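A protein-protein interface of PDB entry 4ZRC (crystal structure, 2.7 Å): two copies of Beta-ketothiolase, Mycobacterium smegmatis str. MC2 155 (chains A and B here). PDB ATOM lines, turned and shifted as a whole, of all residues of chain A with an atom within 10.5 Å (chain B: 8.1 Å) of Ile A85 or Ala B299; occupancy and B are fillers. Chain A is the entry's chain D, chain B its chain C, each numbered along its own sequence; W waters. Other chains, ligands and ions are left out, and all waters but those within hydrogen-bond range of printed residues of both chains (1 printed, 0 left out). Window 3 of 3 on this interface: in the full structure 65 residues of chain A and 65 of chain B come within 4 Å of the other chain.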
ATOM      1  N   ALA A  53      16.134  -0.829 -28.123  1.00  0.00           N
ATOM      2  CA  ALA A  53      15.490  -1.511 -26.992  1.00  0.00           C
ATOM      3  C   ALA A  53      14.084  -2.039 -27.288  1.00  0.00           C
ATOM      4  O   ALA A  53      13.770  -3.152 -26.881  1.00  0.00           O
ATOM      5  CB  ALA A  53      15.497  -0.637 -25.745  1.00  0.00           C
ATOM      6  N   ASP A  54      13.264  -1.283 -28.020  1.00  0.00           N
ATOM      7  CA  ASP A  54      11.892  -1.726 -28.351  1.00  0.00           C
ATOM      8  C   ASP A  54      11.825  -2.877 -29.347  1.00  0.00           C
ATOM      9  O   ASP A  54      10.734  -3.224 -29.820  1.00  0.00           O
ATOM     10  CB  ASP A  54      11.015  -0.558 -28.835  1.00  0.00           C
ATOM     11  CG  ASP A  54      11.518   0.103 -30.152  1.00  0.00           C
ATOM     12  OD1 ASP A  54      12.656  -0.180 -30.629  1.00  0.00           O
ATOM     13  OD2 ASP A  54      10.752   0.940 -30.696  1.00  0.00           O
ATOM     14  N   GLN A  55      12.996  -3.431 -29.670  1.00  0.00           N
ATOM     15  CA  GLN A  55      13.119  -4.561 -30.595  1.00  0.00           C
ATOM     16  C   GLN A  55      12.932  -5.913 -29.867  1.00  0.00           C
ATOM     17  O   GLN A  55      12.344  -6.858 -30.412  1.00  0.00           O
ATOM     18  CB  GLN A  55      14.456  -4.496 -31.377  1.00  0.00           C
ATOM     19  CG  GLN A  55      14.514  -3.431 -32.469  1.00  0.00           C
ATOM     20  CD  GLN A  55      13.472  -3.663 -33.546  1.00  0.00           C
ATOM     21  OE1 GLN A  55      13.588  -4.583 -34.357  1.00  0.00           O
ATOM     22  NE2 GLN A  55      12.442  -2.831 -33.555  1.00  0.00           N
ATOM     23  N   VAL A  56      13.427  -5.976 -28.630  1.00  0.00           N
ATOM     24  CA  VAL A  56      13.254  -7.127 -27.740  1.00  0.00           C
ATOM     25  C   VAL A  56      11.752  -7.381 -27.487  1.00  0.00           C
ATOM     26  O   VAL A  56      11.073  -6.553 -26.893  1.00  0.00           O
ATOM     27  CB  VAL A  56      13.993  -6.891 -26.395  1.00  0.00           C
ATOM     28  CG1 VAL A  56      13.830  -8.079 -25.469  1.00  0.00           C
ATOM     29  CG2 VAL A  56      15.468  -6.579 -26.628  1.00  0.00           C
ATOM     30  N   GLU A  57      11.242  -8.518 -27.942  1.00  0.00           N
ATOM     31  CA  GLU A  57       9.828  -8.837 -27.770  1.00  0.00           C
ATOM     32  C   GLU A  57       9.528  -9.676 -26.516  1.00  0.00           C
ATOM     33  O   GLU A  57       8.373  -9.825 -26.142  1.00  0.00           O
ATOM     34  CB  GLU A  57       9.281  -9.498 -29.025  1.00  0.00           C
ATOM     35  CG  GLU A  57       9.436  -8.635 -30.256  1.00  0.00           C
ATOM     36  CD  GLU A  57       9.001  -9.338 -31.523  1.00  0.00           C
ATOM     37  OE1 GLU A  57       7.774  -9.519 -31.697  1.00  0.00           O
ATOM     38  OE2 GLU A  57       9.879  -9.684 -32.343  1.00  0.00           O
ATOM     39  N   VAL A  59      11.699 -10.855 -22.575  1.00  0.00           N
ATOM     40  CA  VAL A  59      12.822 -11.267 -21.747  1.00  0.00           C
ATOM     41  C   VAL A  59      12.460 -12.511 -20.929  1.00  0.00           C
ATOM     42  O   VAL A  59      11.662 -12.411 -19.982  1.00  0.00           O
ATOM     43  CB  VAL A  59      13.365 -10.144 -20.841  1.00  0.00           C
ATOM     44  CG1 VAL A  59      14.634 -10.615 -20.123  1.00  0.00           C
ATOM     45  CG2 VAL A  59      13.680  -8.917 -21.669  1.00  0.00           C
ATOM     46  N   GLY A  74      11.970 -11.599 -15.501  1.00  0.00           N
ATOM     47  CA  GLY A  74      12.418 -11.145 -16.824  1.00  0.00           C
ATOM     48  C   GLY A  74      11.894  -9.770 -17.186  1.00  0.00           C
ATOM     49  O   GLY A  74      12.547  -8.976 -17.847  1.00  0.00           O
ATOM     50  N   ARG A  75      10.690  -9.493 -16.724  1.00  0.00           N
ATOM     51  CA  ARG A  75      10.061  -8.197 -16.842  1.00  0.00           C
ATOM     52  C   ARG A  75      10.774  -7.234 -15.920  1.00  0.00           C
ATOM     53  O   ARG A  75      11.109  -6.134 -16.331  1.00  0.00           O
ATOM     54  CB  ARG A  75       8.584  -8.338 -16.469  1.00  0.00           C
ATOM     55  CG  ARG A  75       7.839  -7.037 -16.360  1.00  0.00           C
ATOM     56  CD  ARG A  75       7.714  -6.321 -17.683  1.00  0.00           C
ATOM     57  NE  ARG A  75       6.677  -5.308 -17.562  1.00  0.00           N
ATOM     58  CZ  ARG A  75       6.532  -4.266 -18.363  1.00  0.00           C
ATOM     59  NH1 ARG A  75       7.358  -4.031 -19.377  1.00  0.00           N
ATOM     60  NH2 ARG A  75       5.541  -3.439 -18.128  1.00  0.00           N
ATOM     61  N   VAL A  76      11.008  -7.648 -14.683  1.00  0.00           N
ATOM     62  CA  VAL A  76      11.735  -6.818 -13.758  1.00  0.00           C
ATOM     63  C   VAL A  76      13.120  -6.469 -14.298  1.00  0.00           C
ATOM     64  O   VAL A  76      13.439  -5.287 -14.464  1.00  0.00           O
ATOM     65  CB  VAL A  76      11.765  -7.360 -12.324  1.00  0.00           C
ATOM     66  CG1 VAL A  76      12.764  -6.572 -11.480  1.00  0.00           C
ATOM     67  CG2 VAL A  76      10.393  -7.226 -11.721  1.00  0.00           C
ATOM     68  N   ALA A  78      14.210  -6.421 -17.295  1.00  0.00           N
ATOM     69  CA  ALA A  78      14.002  -5.526 -18.426  1.00  0.00           C
ATOM     70  C   ALA A  78      13.769  -3.992 -18.113  1.00  0.00           C
ATOM     71  O   ALA A  78      14.390  -3.103 -18.743  1.00  0.00           O
ATOM     72  CB  ALA A  78      12.887  -6.070 -19.296  1.00  0.00           C
ATOM     73  N   LEU A  79      12.873  -3.689 -17.170  1.00  0.00           N
ATOM     74  CA  LEU A  79      12.610  -2.325 -16.782  1.00  0.00           C
ATOM     75  C   LEU A  79      13.822  -1.758 -16.064  1.00  0.00           C
ATOM     76  O   LEU A  79      14.326  -0.693 -16.401  1.00  0.00           O
ATOM     77  CB  LEU A  79      11.382  -2.268 -15.893  1.00  0.00           C
ATOM     78  CG  LEU A  79      10.083  -2.820 -16.505  1.00  0.00           C
ATOM     79  CD1 LEU A  79       8.970  -2.981 -15.479  1.00  0.00           C
ATOM     80  CD2 LEU A  79       9.570  -1.996 -17.681  1.00  0.00           C
ATOM     81  N   ASP A  80      14.329  -2.504 -15.101  1.00  0.00           N
ATOM     82  CA  ASP A  80      15.434  -2.040 -14.273  1.00  0.00           C
ATOM     83  C   ASP A  80      16.728  -1.789 -15.042  1.00  0.00           C
ATOM     84  O   ASP A  80      17.639  -1.116 -14.526  1.00  0.00           O
ATOM     85  CB  ASP A  80      15.691  -3.009 -13.099  1.00  0.00           C
ATOM     86  CG  ASP A  80      14.804  -2.731 -11.884  1.00  0.00           C
ATOM     87  OD1 ASP A  80      13.698  -2.184 -12.065  1.00  0.00           O
ATOM     88  OD2 ASP A  80      15.230  -3.066 -10.757  1.00  0.00           O
ATOM     89  N   ALA A  81      16.801  -2.332 -16.256  1.00  0.00           N
ATOM     90  CA  ALA A  81      17.981  -2.208 -17.100  1.00  0.00           C
ATOM     91  C   ALA A  81      17.870  -1.095 -18.152  1.00  0.00           C
ATOM     92  O   ALA A  81      18.846  -0.781 -18.830  1.00  0.00           O
ATOM     93  CB  ALA A  81      18.303  -3.547 -17.760  1.00  0.00           C
ATOM     94  N   GLY A  82      16.696  -0.491 -18.287  1.00  0.00           N
ATOM     95  CA  GLY A  82      16.520   0.528 -19.311  1.00  0.00           C
ATOM     96  C   GLY A  82      15.310   0.351 -20.189  1.00  0.00           C
ATOM     97  O   GLY A  82      14.515   1.276 -20.283  1.00  0.00           O
ATOM     98  N   LEU A  83      15.161  -0.827 -20.812  1.00  0.00           N
ATOM     99  CA  LEU A  83      14.146  -1.078 -21.866  1.00  0.00           C
ATOM    100  C   LEU A  83      12.774  -0.395 -21.640  1.00  0.00           C
ATOM    101  O   LEU A  83      12.384  -0.164 -20.498  1.00  0.00           O
ATOM    102  CB  LEU A  83      13.981  -2.585 -22.080  1.00  0.00           C
ATOM    103  CG  LEU A  83      15.186  -3.386 -22.579  1.00  0.00           C
ATOM    104  CD1 LEU A  83      16.260  -3.521 -21.491  1.00  0.00           C
ATOM    105  CD2 LEU A  83      14.759  -4.750 -23.133  1.00  0.00           C
ATOM    106  N   PRO A  84      12.033  -0.079 -22.720  1.00  0.00           N
ATOM    107  CA  PRO A  84      10.719   0.565 -22.553  1.00  0.00           C
ATOM    108  C   PRO A  84       9.576  -0.307 -21.916  1.00  0.00           C
ATOM    109  O   PRO A  84       9.662  -1.552 -21.880  1.00  0.00           O
ATOM    110  CB  PRO A  84      10.363   0.995 -23.990  1.00  0.00           C
ATOM    111  CG  PRO A  84      11.018  -0.028 -24.837  1.00  0.00           C
ATOM    112  CD  PRO A  84      12.329  -0.312 -24.145  1.00  0.00           C
ATOM    113  N   ILE A  85       8.520   0.363 -21.441  1.00  0.00           N
ATOM    114  CA  ILE A  85       7.349  -0.315 -20.866  1.00  0.00           C
ATOM    115  C   ILE A  85       6.616  -1.303 -21.800  1.00  0.00           C
ATOM    116  O   ILE A  85       5.704  -1.960 -21.361  1.00  0.00           O
ATOM    117  CB  ILE A  85       6.326   0.678 -20.241  1.00  0.00           C
ATOM    118  CG1 ILE A  85       5.866   1.735 -21.266  1.00  0.00           C
ATOM    119  CG2 ILE A  85       6.911   1.348 -19.009  1.00  0.00           C
ATOM    120  CD1 ILE A  85       4.389   2.076 -21.220  1.00  0.00           C
ATOM    121  N   THR A  86       7.045  -1.423 -23.055  1.00  0.00           N
ATOM    122  CA  THR A  86       6.396  -2.305 -24.027  1.00  0.00           C
ATOM    123  C   THR A  86       7.006  -3.691 -24.123  1.00  0.00           C
ATOM    124  O   THR A  86       6.395  -4.560 -24.738  1.00  0.00           O
ATOM    125  CB  THR A  86       6.413  -1.714 -25.461  1.00  0.00           C
ATOM    126  OG1 THR A  86       7.722  -1.166 -25.745  1.00  0.00           O
ATOM    127  CG2 THR A  86       5.299  -0.666 -25.646  1.00  0.00           C
ATOM    128  N   VAL A  87       8.216  -3.876 -23.578  1.00  0.00           N
ATOM    129  CA  VAL A  87       8.926  -5.184 -23.569  1.00  0.00           C
ATOM    130  C   VAL A  87       8.345  -6.126 -22.478  1.00  0.00           C
ATOM    131  O   VAL A  87       8.496  -5.832 -21.264  1.00  0.00           O
ATOM    132  CB  VAL A  87      10.454  -5.026 -23.281  1.00  0.00           C
ATOM    133  CG1 VAL A  87      11.181  -6.368 -23.355  1.00  0.00           C
ATOM    134  CG2 VAL A  87      11.112  -4.016 -24.208  1.00  0.00           C
ATOM    135  N   PRO A  88       7.669  -7.235 -22.892  1.00  0.00           N
ATOM    136  CA  PRO A  88       7.232  -8.242 -21.926  1.00  0.00           C
ATOM    137  C   PRO A  88       8.411  -9.047 -21.314  1.00  0.00           C
ATOM    138  O   PRO A  88       9.538  -9.029 -21.847  1.00  0.00           O
ATOM    139  CB  PRO A  88       6.324  -9.152 -22.769  1.00  0.00           C
ATOM    140  CG  PRO A  88       5.931  -8.341 -23.972  1.00  0.00           C
ATOM    141  CD  PRO A  88       7.151  -7.535 -24.245  1.00  0.00           C
ATOM    142  N   GLY A  89       8.145  -9.735 -20.204  1.00  0.00           N
ATOM    143  CA  GLY A  89       9.137 -10.599 -19.544  1.00  0.00           C
ATOM    144  C   GLY A  89       8.534 -11.686 -18.665  1.00  0.00           C
ATOM    145  O   GLY A  89       7.352 -11.631 -18.327  1.00  0.00           O
ATOM    146  N   GLY B 159       6.855  -3.924 -10.830  1.00  0.00           N
ATOM    147  CA  GLY B 159       7.316  -2.954 -11.846  1.00  0.00           C
ATOM    148  C   GLY B 159       8.741  -2.448 -11.625  1.00  0.00           C
ATOM    149  O   GLY B 159       9.204  -1.550 -12.337  1.00  0.00           O
ATOM    150  N   PHE B 162      12.259   1.591 -10.978  1.00  0.00           N
ATOM    151  CA  PHE B 162      11.816   2.798 -11.728  1.00  0.00           C
ATOM    152  C   PHE B 162      10.308   3.036 -11.807  1.00  0.00           C
ATOM    153  O   PHE B 162       9.887   4.043 -12.373  1.00  0.00           O
ATOM    154  CB  PHE B 162      12.415   2.882 -13.156  1.00  0.00           C
ATOM    155  CG  PHE B 162      13.908   2.802 -13.193  1.00  0.00           C
ATOM    156  CD1 PHE B 162      14.681   3.176 -12.075  1.00  0.00           C
ATOM    157  CD2 PHE B 162      14.556   2.357 -14.345  1.00  0.00           C
ATOM    158  CE1 PHE B 162      16.063   3.076 -12.102  1.00  0.00           C
ATOM    159  CE2 PHE B 162      15.942   2.270 -14.385  1.00  0.00           C
ATOM    160  CZ  PHE B 162      16.696   2.629 -13.263  1.00  0.00           C
ATOM    161  N   HIS B 163       9.489   2.126 -11.287  1.00  0.00           N
ATOM    162  CA  HIS B 163       8.021   2.281 -11.407  1.00  0.00           C
ATOM    163  C   HIS B 163       7.280   1.764 -10.168  1.00  0.00           C
ATOM    164  O   HIS B 163       6.364   0.956 -10.318  1.00  0.00           O
ATOM    165  CB  HIS B 163       7.443   1.542 -12.643  1.00  0.00           C
ATOM    166  CG  HIS B 163       7.881   2.070 -13.977  1.00  0.00           C
ATOM    167  ND1 HIS B 163       9.191   2.130 -14.378  1.00  0.00           N
ATOM    168  CD2 HIS B 163       7.168   2.480 -15.043  1.00  0.00           C
ATOM    169  CE1 HIS B 163       9.274   2.603 -15.607  1.00  0.00           C
ATOM    170  NE2 HIS B 163       8.054   2.817 -16.040  1.00  0.00           N
ATOM    171  N   VAL B 165       4.713   1.003  -7.135  1.00  0.00           N
ATOM    172  CA  VAL B 165       3.266   1.224  -6.982  1.00  0.00           C
ATOM    173  C   VAL B 165       2.888   0.733  -5.586  1.00  0.00           C
ATOM    174  O   VAL B 165       2.601  -0.452  -5.410  1.00  0.00           O
ATOM    175  CB  VAL B 165       2.416   0.537  -8.096  1.00  0.00           C
ATOM    176  CG1 VAL B 165       0.939   0.835  -7.912  1.00  0.00           C
ATOM    177  CG2 VAL B 165       2.839   0.988  -9.493  1.00  0.00           C
ATOM    178  N   THR B 172      -3.475   0.495  -9.108  1.00  0.00           N
ATOM    179  CA  THR B 172      -3.496   0.608 -10.581  1.00  0.00           C
ATOM    180  C   THR B 172      -4.909   0.546 -11.150  1.00  0.00           C
ATOM    181  O   THR B 172      -5.168   1.036 -12.232  1.00  0.00           O
ATOM    182  CB  THR B 172      -2.590  -0.436 -11.323  1.00  0.00           C
ATOM    183  OG1 THR B 172      -3.208  -1.728 -11.342  1.00  0.00           O
ATOM    184  CG2 THR B 172      -1.174  -0.522 -10.714  1.00  0.00           C
ATOM    185  N   ALA B 296       2.121  -8.452 -24.476  1.00  0.00           N
ATOM    186  CA  ALA B 296       2.369  -7.009 -24.511  1.00  0.00           C
ATOM    187  C   ALA B 296       2.840  -6.461 -23.169  1.00  0.00           C
ATOM    188  O   ALA B 296       2.587  -7.043 -22.123  1.00  0.00           O
ATOM    189  CB  ALA B 296       1.156  -6.235 -25.039  1.00  0.00           C
ATOM    190  N   GLY B 297       3.557  -5.348 -23.234  1.00  0.00           N
ATOM    191  CA  GLY B 297       3.939  -4.607 -22.048  1.00  0.00           C
ATOM    192  C   GLY B 297       3.264  -3.246 -22.062  1.00  0.00           C
ATOM    193  O   GLY B 297       3.305  -2.534 -23.055  1.00  0.00           O
ATOM    194  N   VAL B 298       2.634  -2.903 -20.949  1.00  0.00           N
ATOM    195  CA  VAL B 298       2.118  -1.558 -20.712  1.00  0.00           C
ATOM    196  C   VAL B 298       2.742  -0.958 -19.443  1.00  0.00           C
ATOM    197  O   VAL B 298       3.618  -1.566 -18.815  1.00  0.00           O
ATOM    198  CB  VAL B 298       0.579  -1.508 -20.651  1.00  0.00           C
ATOM    199  CG1 VAL B 298      -0.018  -1.998 -21.963  1.00  0.00           C
ATOM    200  CG2 VAL B 298       0.045  -2.309 -19.473  1.00  0.00           C
ATOM    201  N   ALA B 299       2.308   0.244 -19.078  1.00  0.00           N
ATOM    202  CA  ALA B 299       2.811   0.871 -17.855  1.00  0.00           C
ATOM    203  C   ALA B 299       2.462  -0.017 -16.645  1.00  0.00           C
ATOM    204  O   ALA B 299       1.349  -0.516 -16.537  1.00  0.00           O
ATOM    205  CB  ALA B 299       2.243   2.272 -17.691  1.00  0.00           C
ATOM    206  N   PRO B 300       3.430  -0.263 -15.759  1.00  0.00           N
ATOM    207  CA  PRO B 300       3.102  -0.883 -14.499  1.00  0.00           C
ATOM    208  C   PRO B 300       1.911  -0.202 -13.788  1.00  0.00           C
ATOM    209  O   PRO B 300       0.979  -0.895 -13.385  1.00  0.00           O
ATOM    210  CB  PRO B 300       4.395  -0.723 -13.693  1.00  0.00           C
ATOM    211  CG  PRO B 300       5.463  -0.736 -14.714  1.00  0.00           C
ATOM    212  CD  PRO B 300       4.882  -0.170 -15.973  1.00  0.00           C
ATOM    213  N   ASP B 301       1.939   1.130 -13.650  1.00  0.00           N
ATOM    214  CA  ASP B 301       0.873   1.890 -12.965  1.00  0.00           C
ATOM    215  C   ASP B 301      -0.490   1.804 -13.693  1.00  0.00           C
ATOM    216  O   ASP B 301      -1.507   2.217 -13.157  1.00  0.00           O
ATOM    217  CB  ASP B 301       1.292   3.363 -12.701  1.00  0.00           C
ATOM    218  CG  ASP B 301       1.498   4.196 -14.008  1.00  0.00           C
ATOM    219  OD1 ASP B 301       1.034   3.781 -15.098  1.00  0.00           O
ATOM    220  OD2 ASP B 301       2.134   5.282 -13.938  1.00  0.00           O
ATOM    221  N   LEU B 302      -0.483   1.261 -14.908  1.00  0.00           N
ATOM    222  CA  LEU B 302      -1.674   1.122 -15.734  1.00  0.00           C
ATOM    223  C   LEU B 302      -1.829  -0.319 -16.219  1.00  0.00           C
ATOM    224  O   LEU B 302      -2.394  -0.555 -17.305  1.00  0.00           O
ATOM    225  CB  LEU B 302      -1.600   2.065 -16.953  1.00  0.00           C
ATOM    226  CG  LEU B 302      -1.811   3.570 -16.767  1.00  0.00           C
ATOM    227  CD1 LEU B 302      -1.358   4.335 -18.015  1.00  0.00           C
ATOM    228  CD2 LEU B 302      -3.251   3.866 -16.362  1.00  0.00           C
ATOM    229  N   MET B 303      -1.343  -1.277 -15.419  1.00  0.00           N
ATOM    230  CA  MET B 303      -1.310  -2.714 -15.810  1.00  0.00           C
ATOM    231  C   MET B 303      -2.657  -3.280 -16.321  1.00  0.00           C
ATOM    232  O   MET B 303      -2.668  -4.111 -17.234  1.00  0.00           O
ATOM    233  CB  MET B 303      -0.694  -3.596 -14.692  1.00  0.00           C
ATOM    234  CG  MET B 303      -1.606  -3.932 -13.497  1.00  0.00           C
ATOM    235  SD  MET B 303      -2.672  -5.388 -13.700  1.00  0.00           S
ATOM    236  CE  MET B 303      -3.989  -5.058 -12.532  1.00  0.00           C
ATOM    237  N   GLY B 304      -3.766  -2.784 -15.752  1.00  0.00           N
ATOM    238  CA  GLY B 304      -5.122  -3.261 -16.030  1.00  0.00           C
ATOM    239  C   GLY B 304      -5.474  -3.316 -17.498  1.00  0.00           C
ATOM    240  O   GLY B 304      -6.301  -4.124 -17.938  1.00  0.00           O
ATOM    241  N   ILE B 305      -4.772  -2.478 -18.253  1.00  0.00           N
ATOM    242  CA  ILE B 305      -5.076  -2.184 -19.642  1.00  0.00           C
ATOM    243  C   ILE B 305      -4.426  -3.193 -20.594  1.00  0.00           C
ATOM    244  O   ILE B 305      -4.758  -3.246 -21.810  1.00  0.00           O
ATOM    245  CB  ILE B 305      -4.750  -0.667 -19.968  1.00  0.00           C
ATOM    246  CG1 ILE B 305      -5.765  -0.073 -20.952  1.00  0.00           C
ATOM    247  CG2 ILE B 305      -3.312  -0.414 -20.406  1.00  0.00           C
ATOM    248  CD1 ILE B 305      -7.188  -0.077 -20.416  1.00  0.00           C
ATOM    249  N   GLY B 306      -3.519  -3.998 -20.021  1.00  0.00           N
ATOM    250  CA  GLY B 306      -2.764  -4.991 -20.765  1.00  0.00           C
ATOM    251  C   GLY B 306      -3.468  -5.787 -21.861  1.00  0.00           C
ATOM    252  O   GLY B 306      -2.846  -6.049 -22.883  1.00  0.00           O
ATOM    253  N   PRO B 309      -3.389  -3.904 -26.053  1.00  0.00           N
ATOM    254  CA  PRO B 309      -2.377  -4.151 -27.096  1.00  0.00           C
ATOM    255  C   PRO B 309      -2.199  -5.630 -27.431  1.00  0.00           C
ATOM    256  O   PRO B 309      -1.890  -5.961 -28.580  1.00  0.00           O
ATOM    257  CB  PRO B 309      -1.088  -3.579 -26.505  1.00  0.00           C
ATOM    258  CG  PRO B 309      -1.350  -3.399 -25.059  1.00  0.00           C
ATOM    259  CD  PRO B 309      -2.813  -3.266 -24.853  1.00  0.00           C
ATOM    260  N   ILE B 397      -1.759  -8.325 -16.193  1.00  0.00           N
ATOM    261  CA  ILE B 397      -0.709  -9.000 -15.494  1.00  0.00           C
ATOM    262  C   ILE B 397       0.044  -7.968 -14.658  1.00  0.00           C
ATOM    263  O   ILE B 397       0.574  -7.006 -15.189  1.00  0.00           O
ATOM    264  CB  ILE B 397       0.245  -9.667 -16.495  1.00  0.00           C
ATOM    265  CG1 ILE B 397      -0.493 -10.672 -17.385  1.00  0.00           C
ATOM    266  CG2 ILE B 397       1.482 -10.239 -15.795  1.00  0.00           C
ATOM    267  CD1 ILE B 397       0.307 -11.096 -18.585  1.00  0.00           C
ATOM    268  N   GLY B 398       0.082  -8.169 -13.347  1.00  0.00           N
ATOM    269  CA  GLY B 398       0.832  -7.300 -12.462  1.00  0.00           C
ATOM    270  C   GLY B 398       2.195  -6.943 -13.014  1.00  0.00           C
ATOM    271  O   GLY B 398       2.845  -7.770 -13.627  1.00  0.00           O
ATOM    272  N   GLY B 399       2.645  -5.718 -12.807  1.00  0.00           N
ATOM    273  CA  GLY B 399       3.932  -5.321 -13.334  1.00  0.00           C
ATOM    274  C   GLY B 399       3.831  -4.771 -14.740  1.00  0.00           C
ATOM    275  O   GLY B 399       4.836  -4.305 -15.288  1.00  0.00           O
ATOM    276  N   GLY B 400       2.645  -4.833 -15.342  1.00  0.00           N
ATOM    277  CA  GLY B 400       2.414  -4.175 -16.615  1.00  0.00           C
ATOM    278  C   GLY B 400       2.658  -5.067 -17.808  1.00  0.00           C
ATOM    279  O   GLY B 400       3.560  -4.819 -18.628  1.00  0.00           O
ATOM    280  N   GLN B 401       1.859  -6.122 -17.903  1.00  0.00           N
ATOM    281  CA  GLN B 401       1.824  -6.975 -19.080  1.00  0.00           C
ATOM    282  C   GLN B 401       0.381  -7.373 -19.363  1.00  0.00           C
ATOM    283  O   GLN B 401      -0.512  -7.157 -18.536  1.00  0.00           O
ATOM    284  CB  GLN B 401       2.681  -8.232 -18.898  1.00  0.00           C
ATOM    285  CG  GLN B 401       4.058  -7.974 -18.319  1.00  0.00           C
ATOM    286  CD  GLN B 401       4.978  -9.176 -18.398  1.00  0.00           C
ATOM    287  OE1 GLN B 401       5.279  -9.668 -19.482  1.00  0.00           O
ATOM    288  NE2 GLN B 401       5.456  -9.634 -17.237  1.00  0.00           N
HETATM  289  O   HOH W   1      12.226  -0.339 -12.546  1.00  0.00           O
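Printed residues of chain B within 4 Å of Leu A79: Gly B159 and Phe B162. Of the printed residues of chain B, Asp A80 touches Phe B162 (3.8 Å). Leu A83 touches none of the printed residues of chain B. Of chain B, only His B163, Gly B297, Val B298, Ala B299 and Pro B300 come within 4 Å of Ile A85. Of the printed residues of chain B, Gly A89 touches Gln B401. Printed residues of chain A within 4 Å of Gly B159: Leu A79 (3.5 Å). Of the printed residues of chain A, His B163 touches Ile A85 (3.5 Å). Of chain A, only Ile A85 (2.8 Å), Thr A86 (3.2 Å) and Pro A88 (3.9 Å) come within 4 Å of Gly B297. Ala B299 touches one residue of chain A. Pro B300 touches just these residues of chain A: Arg A75 (3.97 Å) and Ile A85 (3.95 Å). No residue of chain A comes within 4 Å of Leu B302. Ile B305 touches none of the printed residues of chain A. The nearest residue of chain A that does not touch Ala B299 is Arg A75 (4.8 Å). The nearest printed residue of chain A that does not touch Ala B296 is Thr A86 (4.3 Å).
The backbone carbonyl oxygen of Gly B400 is in hydrogen-bond range of the guanidinium group of Arg A75 (2.5 Å). The backbone NH of Val B298 lies within hydrogen-bond range of the backbone carbonyl oxygen of Ile A85 (3.2 Å). The backbone NH (N) of Gly B297 sits at hydrogen-bond distance from the backbone carbonyl oxygen (O) of Thr A86 (3.3 Å). O of Gly B399 lies within hydrogen-bond range of NH2 of Arg A75 (3.1 Å). The backbone carbonyl oxygen (O) of Val B298 sits at hydrogen-bond distance from the guanidinium group (NH2) of Arg A75, 2.8 Å away. The side-chain amide oxygen of Gln B401 lies within hydrogen-bond range of the backbone NH of Gly A89. The backbone carbonyl oxygen of Ile A85 lies close to the backbone carbonyl oxygen of Gly B297, 3.0 Å away.
No position is printed for both chains. Of the 18 pairs that touch across the chains among the printed residues, none has its exchanged pair printed and touching as well.
Arg A75 touches Pro B300 (NH2 to CD, 3.97 Å). Leu A79 touches Gly B159. Leu A79 touches Phe B162 (O to CD2, 3.7 Å). CE2 of Phe B162 touches O of Asp A80 (3.8 Å). CG2 of Ile A85 touches NE2 of His B163, at 3.5 Å. Ala B299 touches Ile A85 (N to CD1, 3.5 Å). CD of Pro B300 touches CG2 of Ile A85, at 3.95 Å. C of Ala B296 touches CG of Pro A88, 3.7 Å away. Pro A88 touches Gly B297 (CG to N, 3.9 Å). CA of Pro A88 touches OE1 of Gln B401 (3.4 Å).
Water W1 lies within hydrogen-bond range of OD1 of Asp A80 (2.4 Å), N of Phe B162 (2.5 Å) and O of Gly B159 (3.3 Å).
The backbone carbonyl oxygen (O) of Pro A88 is in hydrogen-bond range of the backbone NH (N) of Val A59, 2.9 Å away. The backbone carbonyl oxygen (O) of Ile A85 is in hydrogen-bond range of the guanidinium group (NH1) of Arg A75, 3.3 Å away. NH1 of Arg A75 lies within hydrogen-bond range of O of Val A87 (2.8 Å). The backbone NH (N) of Val B298 sits at hydrogen-bond distance from the backbone carbonyl oxygen (O) of Gly B400 (3.1 Å).
Of the 22 printed residues of chain B, 11 touch a printed residue of chain A. Hydrophobic or aromatic side chains of chain B that line the printed part of chain A: Phe B162, His B163 and Pro B300. Printed residues of chain A that touch a printed residue of chain B: Arg A75, Leu A79, Asp A80, Ile A85, Thr A86, Pro A88 and Gly A89. Hydrophobic or aromatic side chains of chain A that line the printed part of chain B: Leu A79, Ile A85 and Pro A88. Among the printed residues, 18 pairs touch across the chains.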
